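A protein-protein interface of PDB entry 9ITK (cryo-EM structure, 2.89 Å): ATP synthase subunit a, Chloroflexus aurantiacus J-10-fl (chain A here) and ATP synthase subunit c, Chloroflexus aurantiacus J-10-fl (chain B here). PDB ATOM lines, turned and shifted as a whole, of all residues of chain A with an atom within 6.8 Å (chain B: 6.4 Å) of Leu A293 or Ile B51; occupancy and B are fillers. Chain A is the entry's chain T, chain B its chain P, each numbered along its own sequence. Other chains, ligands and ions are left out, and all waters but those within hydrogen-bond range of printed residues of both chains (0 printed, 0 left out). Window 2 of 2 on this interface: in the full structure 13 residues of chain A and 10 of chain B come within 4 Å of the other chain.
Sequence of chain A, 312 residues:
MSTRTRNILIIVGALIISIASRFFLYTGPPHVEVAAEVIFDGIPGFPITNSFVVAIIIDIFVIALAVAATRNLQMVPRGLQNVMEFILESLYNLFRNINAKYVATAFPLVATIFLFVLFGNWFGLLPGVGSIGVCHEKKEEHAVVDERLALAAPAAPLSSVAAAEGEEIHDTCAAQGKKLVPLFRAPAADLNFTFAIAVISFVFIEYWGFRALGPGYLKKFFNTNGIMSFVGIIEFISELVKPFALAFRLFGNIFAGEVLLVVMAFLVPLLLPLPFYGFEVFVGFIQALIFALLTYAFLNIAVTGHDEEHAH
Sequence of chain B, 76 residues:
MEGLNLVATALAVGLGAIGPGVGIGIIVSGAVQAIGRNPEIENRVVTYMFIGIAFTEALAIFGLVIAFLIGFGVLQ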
ATOM      1  N   LEU A  91       6.209 -10.978 -20.895  1.00  0.00           N
ATOM      2  CA  LEU A  91       7.297 -11.923 -21.115  1.00  0.00           C
ATOM      3  C   LEU A  91       7.603 -12.063 -22.599  1.00  0.00           C
ATOM      4  O   LEU A  91       8.772 -12.150 -22.991  1.00  0.00           O
ATOM      5  CB  LEU A  91       6.955 -13.283 -20.506  1.00  0.00           C
ATOM      6  CG  LEU A  91       7.273 -13.509 -19.025  1.00  0.00           C
ATOM      7  CD1 LEU A  91       8.773 -13.439 -18.799  1.00  0.00           C
ATOM      8  CD2 LEU A  91       6.547 -12.519 -18.126  1.00  0.00           C
ATOM      9  N   LEU A  94       9.779  -9.305 -23.583  1.00  0.00           N
ATOM     10  CA  LEU A  94      11.136  -9.421 -23.054  1.00  0.00           C
ATOM     11  C   LEU A  94      11.984 -10.354 -23.909  1.00  0.00           C
ATOM     12  O   LEU A  94      13.140 -10.051 -24.222  1.00  0.00           O
ATOM     13  CB  LEU A  94      11.094  -9.913 -21.608  1.00  0.00           C
ATOM     14  CG  LEU A  94      11.248  -8.872 -20.499  1.00  0.00           C
ATOM     15  CD1 LEU A  94      10.253  -7.736 -20.672  1.00  0.00           C
ATOM     16  CD2 LEU A  94      11.086  -9.527 -19.140  1.00  0.00           C
ATOM     17  N   PHE A  95      11.423 -11.501 -24.296  1.00  0.00           N
ATOM     18  CA  PHE A  95      12.191 -12.463 -25.077  1.00  0.00           C
ATOM     19  C   PHE A  95      12.428 -11.960 -26.494  1.00  0.00           C
ATOM     20  O   PHE A  95      13.476 -12.236 -27.090  1.00  0.00           O
ATOM     21  CB  PHE A  95      11.475 -13.813 -25.093  1.00  0.00           C
ATOM     22  CG  PHE A  95      11.239 -14.379 -23.727  1.00  0.00           C
ATOM     23  CD1 PHE A  95      12.258 -14.411 -22.794  1.00  0.00           C
ATOM     24  CD2 PHE A  95       9.997 -14.871 -23.373  1.00  0.00           C
ATOM     25  CE1 PHE A  95      12.042 -14.927 -21.534  1.00  0.00           C
ATOM     26  CE2 PHE A  95       9.774 -15.384 -22.112  1.00  0.00           C
ATOM     27  CZ  PHE A  95      10.798 -15.414 -21.192  1.00  0.00           C
ATOM     28  N   ILE A  98      15.529  -9.719 -26.581  1.00  0.00           N
ATOM     29  CA  ILE A  98      16.782 -10.469 -26.606  1.00  0.00           C
ATOM     30  C   ILE A  98      17.023 -11.052 -27.992  1.00  0.00           C
ATOM     31  O   ILE A  98      18.127 -10.962 -28.541  1.00  0.00           O
ATOM     32  CB  ILE A  98      16.768 -11.566 -25.527  1.00  0.00           C
ATOM     33  CG1 ILE A  98      16.660 -10.943 -24.138  1.00  0.00           C
ATOM     34  CG2 ILE A  98      18.021 -12.417 -25.618  1.00  0.00           C
ATOM     35  CD1 ILE A  98      16.236 -11.919 -23.077  1.00  0.00           C
ATOM     36  N   VAL A 110       9.905 -21.457 -21.719  1.00  0.00           N
ATOM     37  CA  VAL A 110      10.226 -20.377 -20.792  1.00  0.00           C
ATOM     38  C   VAL A 110       8.974 -19.875 -20.084  1.00  0.00           C
ATOM     39  O   VAL A 110       9.004 -19.570 -18.885  1.00  0.00           O
ATOM     40  CB  VAL A 110      10.964 -19.242 -21.525  1.00  0.00           C
ATOM     41  CG1 VAL A 110      12.349 -19.696 -21.929  1.00  0.00           C
ATOM     42  CG2 VAL A 110      10.188 -18.799 -22.740  1.00  0.00           C
ATOM     43  N   ILE A 113       8.208 -22.130 -17.482  1.00  0.00           N
ATOM     44  CA  ILE A 113       9.222 -21.951 -16.445  1.00  0.00           C
ATOM     45  C   ILE A 113       8.873 -20.762 -15.560  1.00  0.00           C
ATOM     46  O   ILE A 113       8.889 -20.857 -14.329  1.00  0.00           O
ATOM     47  CB  ILE A 113      10.618 -21.795 -17.077  1.00  0.00           C
ATOM     48  CG1 ILE A 113      11.199 -23.151 -17.472  1.00  0.00           C
ATOM     49  CG2 ILE A 113      11.557 -21.075 -16.143  1.00  0.00           C
ATOM     50  CD1 ILE A 113      12.610 -23.054 -18.007  1.00  0.00           C
ATOM     51  N   ARG A 249      21.457 -21.911  -8.246  1.00  0.00           N
ATOM     52  CA  ARG A 249      20.980 -20.552  -8.014  1.00  0.00           C
ATOM     53  C   ARG A 249      19.526 -20.548  -7.561  1.00  0.00           C
ATOM     54  O   ARG A 249      19.154 -19.819  -6.635  1.00  0.00           O
ATOM     55  CB  ARG A 249      21.150 -19.718  -9.281  1.00  0.00           C
ATOM     56  CG  ARG A 249      20.767 -18.261  -9.127  1.00  0.00           C
ATOM     57  CD  ARG A 249      20.393 -17.652 -10.465  1.00  0.00           C
ATOM     58  NE  ARG A 249      21.183 -18.208 -11.558  1.00  0.00           N
ATOM     59  CZ  ARG A 249      22.439 -17.875 -11.821  1.00  0.00           C
ATOM     60  NH1 ARG A 249      23.085 -16.985 -11.088  1.00  0.00           N
ATOM     61  NH2 ARG A 249      23.062 -18.452 -12.844  1.00  0.00           N
ATOM     62  N   ILE A 286      11.915 -12.645  -8.788  1.00  0.00           N
ATOM     63  CA  ILE A 286      13.087 -12.361  -9.613  1.00  0.00           C
ATOM     64  C   ILE A 286      13.752 -13.652 -10.069  1.00  0.00           C
ATOM     65  O   ILE A 286      14.112 -13.799 -11.244  1.00  0.00           O
ATOM     66  CB  ILE A 286      14.068 -11.454  -8.851  1.00  0.00           C
ATOM     67  CG1 ILE A 286      13.482 -10.052  -8.707  1.00  0.00           C
ATOM     68  CG2 ILE A 286      15.404 -11.396  -9.567  1.00  0.00           C
ATOM     69  CD1 ILE A 286      13.352  -9.313 -10.014  1.00  0.00           C
ATOM     70  N   ALA A 288      12.300 -16.446 -10.458  1.00  0.00           N
ATOM     71  CA  ALA A 288      11.408 -16.965 -11.486  1.00  0.00           C
ATOM     72  C   ALA A 288      11.634 -16.260 -12.817  1.00  0.00           C
ATOM     73  O   ALA A 288      11.685 -16.906 -13.870  1.00  0.00           O
ATOM     74  CB  ALA A 288       9.956 -16.813 -11.041  1.00  0.00           C
ATOM     75  N   LEU A 289      11.784 -14.935 -12.788  1.00  0.00           N
ATOM     76  CA  LEU A 289      11.890 -14.178 -14.029  1.00  0.00           C
ATOM     77  C   LEU A 289      13.231 -14.408 -14.715  1.00  0.00           C
ATOM     78  O   LEU A 289      13.281 -14.592 -15.937  1.00  0.00           O
ATOM     79  CB  LEU A 289      11.667 -12.692 -13.754  1.00  0.00           C
ATOM     80  CG  LEU A 289      11.481 -11.789 -14.973  1.00  0.00           C
ATOM     81  CD1 LEU A 289      10.452 -10.723 -14.670  1.00  0.00           C
ATOM     82  CD2 LEU A 289      12.798 -11.145 -15.372  1.00  0.00           C
ATOM     83  N   ILE A 290      14.329 -14.397 -13.954  1.00  0.00           N
ATOM     84  CA  ILE A 290      15.646 -14.548 -14.566  1.00  0.00           C
ATOM     85  C   ILE A 290      15.815 -15.948 -15.134  1.00  0.00           C
ATOM     86  O   ILE A 290      16.388 -16.128 -16.215  1.00  0.00           O
ATOM     87  CB  ILE A 290      16.762 -14.229 -13.557  1.00  0.00           C
ATOM     88  CG1 ILE A 290      16.706 -15.211 -12.391  1.00  0.00           C
ATOM     89  CG2 ILE A 290      16.648 -12.800 -13.071  1.00  0.00           C
ATOM     90  CD1 ILE A 290      17.873 -15.143 -11.484  1.00  0.00           C
ATOM     91  N   PHE A 291      15.317 -16.962 -14.424  1.00  0.00           N
ATOM     92  CA  PHE A 291      15.625 -18.338 -14.789  1.00  0.00           C
ATOM     93  C   PHE A 291      15.084 -18.651 -16.176  1.00  0.00           C
ATOM     94  O   PHE A 291      15.753 -19.298 -16.987  1.00  0.00           O
ATOM     95  CB  PHE A 291      15.059 -19.290 -13.738  1.00  0.00           C
ATOM     96  CG  PHE A 291      15.371 -20.734 -13.996  1.00  0.00           C
ATOM     97  CD1 PHE A 291      16.636 -21.231 -13.741  1.00  0.00           C
ATOM     98  CD2 PHE A 291      14.410 -21.588 -14.490  1.00  0.00           C
ATOM     99  CE1 PHE A 291      16.929 -22.555 -13.969  1.00  0.00           C
ATOM    100  CE2 PHE A 291      14.701 -22.914 -14.725  1.00  0.00           C
ATOM    101  CZ  PHE A 291      15.963 -23.398 -14.457  1.00  0.00           C
ATOM    102  N   ALA A 292      13.870 -18.181 -16.470  1.00  0.00           N
ATOM    103  CA  ALA A 292      13.383 -18.210 -17.843  1.00  0.00           C
ATOM    104  C   ALA A 292      14.214 -17.299 -18.736  1.00  0.00           C
ATOM    105  O   ALA A 292      14.519 -17.649 -19.881  1.00  0.00           O
ATOM    106  CB  ALA A 292      11.910 -17.803 -17.885  1.00  0.00           C
ATOM    107  N   LEU A 293      14.597 -16.128 -18.223  1.00  0.00           N
ATOM    108  CA  LEU A 293      15.341 -15.164 -19.029  1.00  0.00           C
ATOM    109  C   LEU A 293      16.721 -15.696 -19.393  1.00  0.00           C
ATOM    110  O   LEU A 293      17.175 -15.525 -20.530  1.00  0.00           O
ATOM    111  CB  LEU A 293      15.439 -13.836 -18.275  1.00  0.00           C
ATOM    112  CG  LEU A 293      15.661 -12.521 -19.026  1.00  0.00           C
ATOM    113  CD1 LEU A 293      15.448 -11.357 -18.077  1.00  0.00           C
ATOM    114  CD2 LEU A 293      17.050 -12.441 -19.627  1.00  0.00           C
ATOM    115  N   LEU A 294      17.405 -16.343 -18.446  1.00  0.00           N
ATOM    116  CA  LEU A 294      18.725 -16.895 -18.739  1.00  0.00           C
ATOM    117  C   LEU A 294      18.665 -17.971 -19.812  1.00  0.00           C
ATOM    118  O   LEU A 294      19.529 -18.019 -20.695  1.00  0.00           O
ATOM    119  CB  LEU A 294      19.376 -17.450 -17.472  1.00  0.00           C
ATOM    120  CG  LEU A 294      20.160 -16.466 -16.608  1.00  0.00           C
ATOM    121  CD1 LEU A 294      21.313 -15.985 -17.455  1.00  0.00           C
ATOM    122  CD2 LEU A 294      19.344 -15.294 -16.104  1.00  0.00           C
ATOM    123  N   THR A 295      17.663 -18.848 -19.752  1.00  0.00           N
ATOM    124  CA  THR A 295      17.568 -19.913 -20.744  1.00  0.00           C
ATOM    125  C   THR A 295      17.427 -19.343 -22.147  1.00  0.00           C
ATOM    126  O   THR A 295      18.069 -19.824 -23.089  1.00  0.00           O
ATOM    127  CB  THR A 295      16.397 -20.835 -20.420  1.00  0.00           C
ATOM    128  OG1 THR A 295      15.179 -20.084 -20.455  1.00  0.00           O
ATOM    129  CG2 THR A 295      16.574 -21.443 -19.048  1.00  0.00           C
ATOM    130  N   TYR A 296      16.595 -18.316 -22.310  1.00  0.00           N
ATOM    131  CA  TYR A 296      16.517 -17.641 -23.600  1.00  0.00           C
ATOM    132  C   TYR A 296      17.816 -16.911 -23.910  1.00  0.00           C
ATOM    133  O   TYR A 296      18.299 -16.949 -25.047  1.00  0.00           O
ATOM    134  CB  TYR A 296      15.326 -16.682 -23.618  1.00  0.00           C
ATOM    135  CG  TYR A 296      14.939 -16.207 -24.999  1.00  0.00           C
ATOM    136  CD1 TYR A 296      15.727 -15.297 -25.692  1.00  0.00           C
ATOM    137  CD2 TYR A 296      13.794 -16.682 -25.619  1.00  0.00           C
ATOM    138  CE1 TYR A 296      15.379 -14.865 -26.953  1.00  0.00           C
ATOM    139  CE2 TYR A 296      13.439 -16.258 -26.882  1.00  0.00           C
ATOM    140  CZ  TYR A 296      14.235 -15.349 -27.544  1.00  0.00           C
ATOM    141  OH  TYR A 296      13.885 -14.922 -28.804  1.00  0.00           O
ATOM    142  N   ALA A 297      18.398 -16.243 -22.912  1.00  0.00           N
ATOM    143  CA  ALA A 297      19.654 -15.535 -23.130  1.00  0.00           C
ATOM    144  C   ALA A 297      20.771 -16.499 -23.501  1.00  0.00           C
ATOM    145  O   ALA A 297      21.595 -16.202 -24.374  1.00  0.00           O
ATOM    146  CB  ALA A 297      20.028 -14.731 -21.886  1.00  0.00           C
ATOM    147  N   PHE A 298      20.820 -17.658 -22.842  1.00  0.00           N
ATOM    148  CA  PHE A 298      21.797 -18.675 -23.214  1.00  0.00           C
ATOM    149  C   PHE A 298      21.470 -19.298 -24.562  1.00  0.00           C
ATOM    150  O   PHE A 298      22.380 -19.713 -25.287  1.00  0.00           O
ATOM    151  CB  PHE A 298      21.876 -19.749 -22.132  1.00  0.00           C
ATOM    152  CG  PHE A 298      22.523 -19.280 -20.865  1.00  0.00           C
ATOM    153  CD1 PHE A 298      23.603 -18.418 -20.905  1.00  0.00           C
ATOM    154  CD2 PHE A 298      22.048 -19.693 -19.635  1.00  0.00           C
ATOM    155  CE1 PHE A 298      24.202 -17.983 -19.744  1.00  0.00           C
ATOM    156  CE2 PHE A 298      22.642 -19.261 -18.469  1.00  0.00           C
ATOM    157  CZ  PHE A 298      23.721 -18.404 -18.524  1.00  0.00           C
ATOM    158  N   LEU A 299      20.185 -19.387 -24.909  1.00  0.00           N
ATOM    159  CA  LEU A 299      19.817 -19.862 -26.236  1.00  0.00           C
ATOM    160  C   LEU A 299      20.293 -18.898 -27.315  1.00  0.00           C
ATOM    161  O   LEU A 299      20.781 -19.326 -28.366  1.00  0.00           O
ATOM    162  CB  LEU A 299      18.305 -20.060 -26.322  1.00  0.00           C
ATOM    163  CG  LEU A 299      17.725 -20.205 -27.730  1.00  0.00           C
ATOM    164  CD1 LEU A 299      18.228 -21.480 -28.379  1.00  0.00           C
ATOM    165  CD2 LEU A 299      16.209 -20.186 -27.688  1.00  0.00           C
ATOM    166  N   VAL B  46      16.948  -1.579 -17.018  1.00  0.00           N
ATOM    167  CA  VAL B  46      16.683  -2.108 -15.687  1.00  0.00           C
ATOM    168  C   VAL B  46      16.534  -3.619 -15.697  1.00  0.00           C
ATOM    169  O   VAL B  46      16.925  -4.284 -14.732  1.00  0.00           O
ATOM    170  CB  VAL B  46      15.434  -1.429 -15.093  1.00  0.00           C
ATOM    171  CG1 VAL B  46      14.972  -2.161 -13.853  1.00  0.00           C
ATOM    172  CG2 VAL B  46      15.754   0.010 -14.753  1.00  0.00           C
ATOM    173  N   THR B  47      15.985  -4.187 -16.770  1.00  0.00           N
ATOM    174  CA  THR B  47      15.911  -5.640 -16.866  1.00  0.00           C
ATOM    175  C   THR B  47      17.293  -6.265 -16.735  1.00  0.00           C
ATOM    176  O   THR B  47      17.440  -7.345 -16.154  1.00  0.00           O
ATOM    177  CB  THR B  47      15.259  -6.053 -18.186  1.00  0.00           C
ATOM    178  OG1 THR B  47      16.184  -5.844 -19.261  1.00  0.00           O
ATOM    179  CG2 THR B  47      14.000  -5.237 -18.433  1.00  0.00           C
ATOM    180  N   TYR B  48      18.320  -5.591 -17.254  1.00  0.00           N
ATOM    181  CA  TYR B  48      19.689  -6.063 -17.080  1.00  0.00           C
ATOM    182  C   TYR B  48      20.220  -5.811 -15.676  1.00  0.00           C
ATOM    183  O   TYR B  48      21.147  -6.505 -15.247  1.00  0.00           O
ATOM    184  CB  TYR B  48      20.605  -5.403 -18.109  1.00  0.00           C
ATOM    185  CG  TYR B  48      20.339  -5.846 -19.528  1.00  0.00           C
ATOM    186  CD1 TYR B  48      19.573  -6.973 -19.792  1.00  0.00           C
ATOM    187  CD2 TYR B  48      20.842  -5.130 -20.602  1.00  0.00           C
ATOM    188  CE1 TYR B  48      19.327  -7.381 -21.083  1.00  0.00           C
ATOM    189  CE2 TYR B  48      20.597  -5.527 -21.895  1.00  0.00           C
ATOM    190  CZ  TYR B  48      19.843  -6.655 -22.132  1.00  0.00           C
ATOM    191  OH  TYR B  48      19.598  -7.056 -23.424  1.00  0.00           O
ATOM    192  N   MET B  49      19.667  -4.830 -14.958  1.00  0.00           N
ATOM    193  CA  MET B  49      20.072  -4.607 -13.574  1.00  0.00           C
ATOM    194  C   MET B  49      19.779  -5.830 -12.715  1.00  0.00           C
ATOM    195  O   MET B  49      20.647  -6.311 -11.980  1.00  0.00           O
ATOM    196  CB  MET B  49      19.359  -3.380 -13.006  1.00  0.00           C
ATOM    197  CG  MET B  49      19.741  -3.055 -11.576  1.00  0.00           C
ATOM    198  SD  MET B  49      18.456  -2.147 -10.697  1.00  0.00           S
ATOM    199  CE  MET B  49      18.959  -0.460 -11.005  1.00  0.00           C
ATOM    200  N   PHE B  50      18.555  -6.351 -12.802  1.00  0.00           N
ATOM    201  CA  PHE B  50      18.156  -7.455 -11.941  1.00  0.00           C
ATOM    202  C   PHE B  50      18.752  -8.784 -12.379  1.00  0.00           C
ATOM    203  O   PHE B  50      18.832  -9.707 -11.562  1.00  0.00           O
ATOM    204  CB  PHE B  50      16.634  -7.537 -11.876  1.00  0.00           C
ATOM    205  CG  PHE B  50      16.020  -6.513 -10.969  1.00  0.00           C
ATOM    206  CD1 PHE B  50      16.370  -6.461  -9.632  1.00  0.00           C
ATOM    207  CD2 PHE B  50      15.115  -5.589 -11.454  1.00  0.00           C
ATOM    208  CE1 PHE B  50      15.816  -5.518  -8.793  1.00  0.00           C
ATOM    209  CE2 PHE B  50      14.559  -4.643 -10.619  1.00  0.00           C
ATOM    210  CZ  PHE B  50      14.911  -4.608  -9.286  1.00  0.00           C
ATOM    211  N   ILE B  51      19.167  -8.912 -13.639  1.00  0.00           N
ATOM    212  CA  ILE B  51      19.944 -10.082 -14.038  1.00  0.00           C
ATOM    213  C   ILE B  51      21.295 -10.078 -13.332  1.00  0.00           C
ATOM    214  O   ILE B  51      21.746 -11.101 -12.804  1.00  0.00           O
ATOM    215  CB  ILE B  51      20.107 -10.136 -15.568  1.00  0.00           C
ATOM    216  CG1 ILE B  51      18.745 -10.201 -16.255  1.00  0.00           C
ATOM    217  CG2 ILE B  51      20.956 -11.321 -15.977  1.00  0.00           C
ATOM    218  CD1 ILE B  51      18.786  -9.785 -17.705  1.00  0.00           C
ATOM    219  N   GLY B  52      21.958  -8.921 -13.314  1.00  0.00           N
ATOM    220  CA  GLY B  52      23.240  -8.827 -12.635  1.00  0.00           C
ATOM    221  C   GLY B  52      23.120  -8.956 -11.129  1.00  0.00           C
ATOM    222  O   GLY B  52      23.955  -9.598 -10.487  1.00  0.00           O
ATOM    223  N   ILE B  53      22.084  -8.350 -10.546  1.00  0.00           N
ATOM    224  CA  ILE B  53      21.886  -8.441  -9.102  1.00  0.00           C
ATOM    225  C   ILE B  53      21.674  -9.890  -8.688  1.00  0.00           C
ATOM    226  O   ILE B  53      22.216 -10.351  -7.677  1.00  0.00           O
ATOM    227  CB  ILE B  53      20.710  -7.550  -8.661  1.00  0.00           C
ATOM    228  CG1 ILE B  53      21.112  -6.078  -8.688  1.00  0.00           C
ATOM    229  CG2 ILE B  53      20.229  -7.938  -7.278  1.00  0.00           C
ATOM    230  CD1 ILE B  53      20.008  -5.147  -8.253  1.00  0.00           C
ATOM    231  N   ALA B  54      20.884 -10.629  -9.464  1.00  0.00           N
ATOM    232  CA  ALA B  54      20.636 -12.027  -9.143  1.00  0.00           C
ATOM    233  C   ALA B  54      21.893 -12.872  -9.308  1.00  0.00           C
ATOM    234  O   ALA B  54      22.112 -13.817  -8.543  1.00  0.00           O
ATOM    235  CB  ALA B  54      19.507 -12.561 -10.012  1.00  0.00           C
ATOM    236  N   PHE B  55      22.725 -12.558 -10.305  1.00  0.00           N
ATOM    237  CA  PHE B  55      24.003 -13.250 -10.448  1.00  0.00           C
ATOM    238  C   PHE B  55      24.881 -13.056  -9.219  1.00  0.00           C
ATOM    239  O   PHE B  55      25.407 -14.024  -8.659  1.00  0.00           O
ATOM    240  CB  PHE B  55      24.735 -12.755 -11.693  1.00  0.00           C
ATOM    241  CG  PHE B  55      24.145 -13.231 -12.976  1.00  0.00           C
ATOM    242  CD1 PHE B  55      23.280 -14.306 -13.000  1.00  0.00           C
ATOM    243  CD2 PHE B  55      24.460 -12.601 -14.163  1.00  0.00           C
ATOM    244  CE1 PHE B  55      22.748 -14.746 -14.188  1.00  0.00           C
ATOM    245  CE2 PHE B  55      23.930 -13.036 -15.350  1.00  0.00           C
ATOM    246  CZ  PHE B  55      23.075 -14.107 -15.362  1.00  0.00           C
ATOM    247  N   THR B  56      25.066 -11.805  -8.798  1.00  0.00           N
ATOM    248  CA  THR B  56      25.877 -11.540  -7.617  1.00  0.00           C
ATOM    249  C   THR B  56      25.247 -12.148  -6.372  1.00  0.00           C
ATOM    250  O   THR B  56      25.934 -12.792  -5.571  1.00  0.00           O
ATOM    251  CB  THR B  56      26.063 -10.038  -7.439  1.00  0.00           C
ATOM    252  OG1 THR B  56      24.781  -9.421  -7.282  1.00  0.00           O
ATOM    253  CG2 THR B  56      26.747  -9.444  -8.652  1.00  0.00           C
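CD1 of Phe B55 touches NH1 of Arg A249, at 3.3 Å. Phe B50 touches Ile A286. Ala B54 touches Ile A290. Ile B51 touches Leu A293. Leu A294 touches Phe B55 (CD1 to CZ, 3.3 Å).
Ile B51 touches one residue of chain A. Of the printed residues of chain B, Ile A286 touches Phe B50 (3.98 Å). Printed residues of chain B within 4 Å of Leu A294: Phe B55. The nearest residue of chain B that does not touch Leu A293 is Thr B47 (4.9 Å). The nearest residue of chain A that does not touch Ile B51 is Leu A294 (4.3 Å). The nearest printed residue of chain A that does not touch Phe B55 is Phe A298 (5.4 Å).
Of the 20 printed residues of chain A, 5 touch a printed residue of chain B. Of the 11 printed residues of chain B, 4 touch a printed residue of chain A. Hydrophobic or aromatic side chains of chain B that line the printed part of chain A: Phe B50, Ile B51, Ala B54 and Phe B55. Along chain B the printed residues that touch a printed residue of chain A span positions 50 to 55. Among the printed residues, no Asp or Glu carboxylate lies within 4 Å of a Lys or Arg side-chain nitrogen of the other chain.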
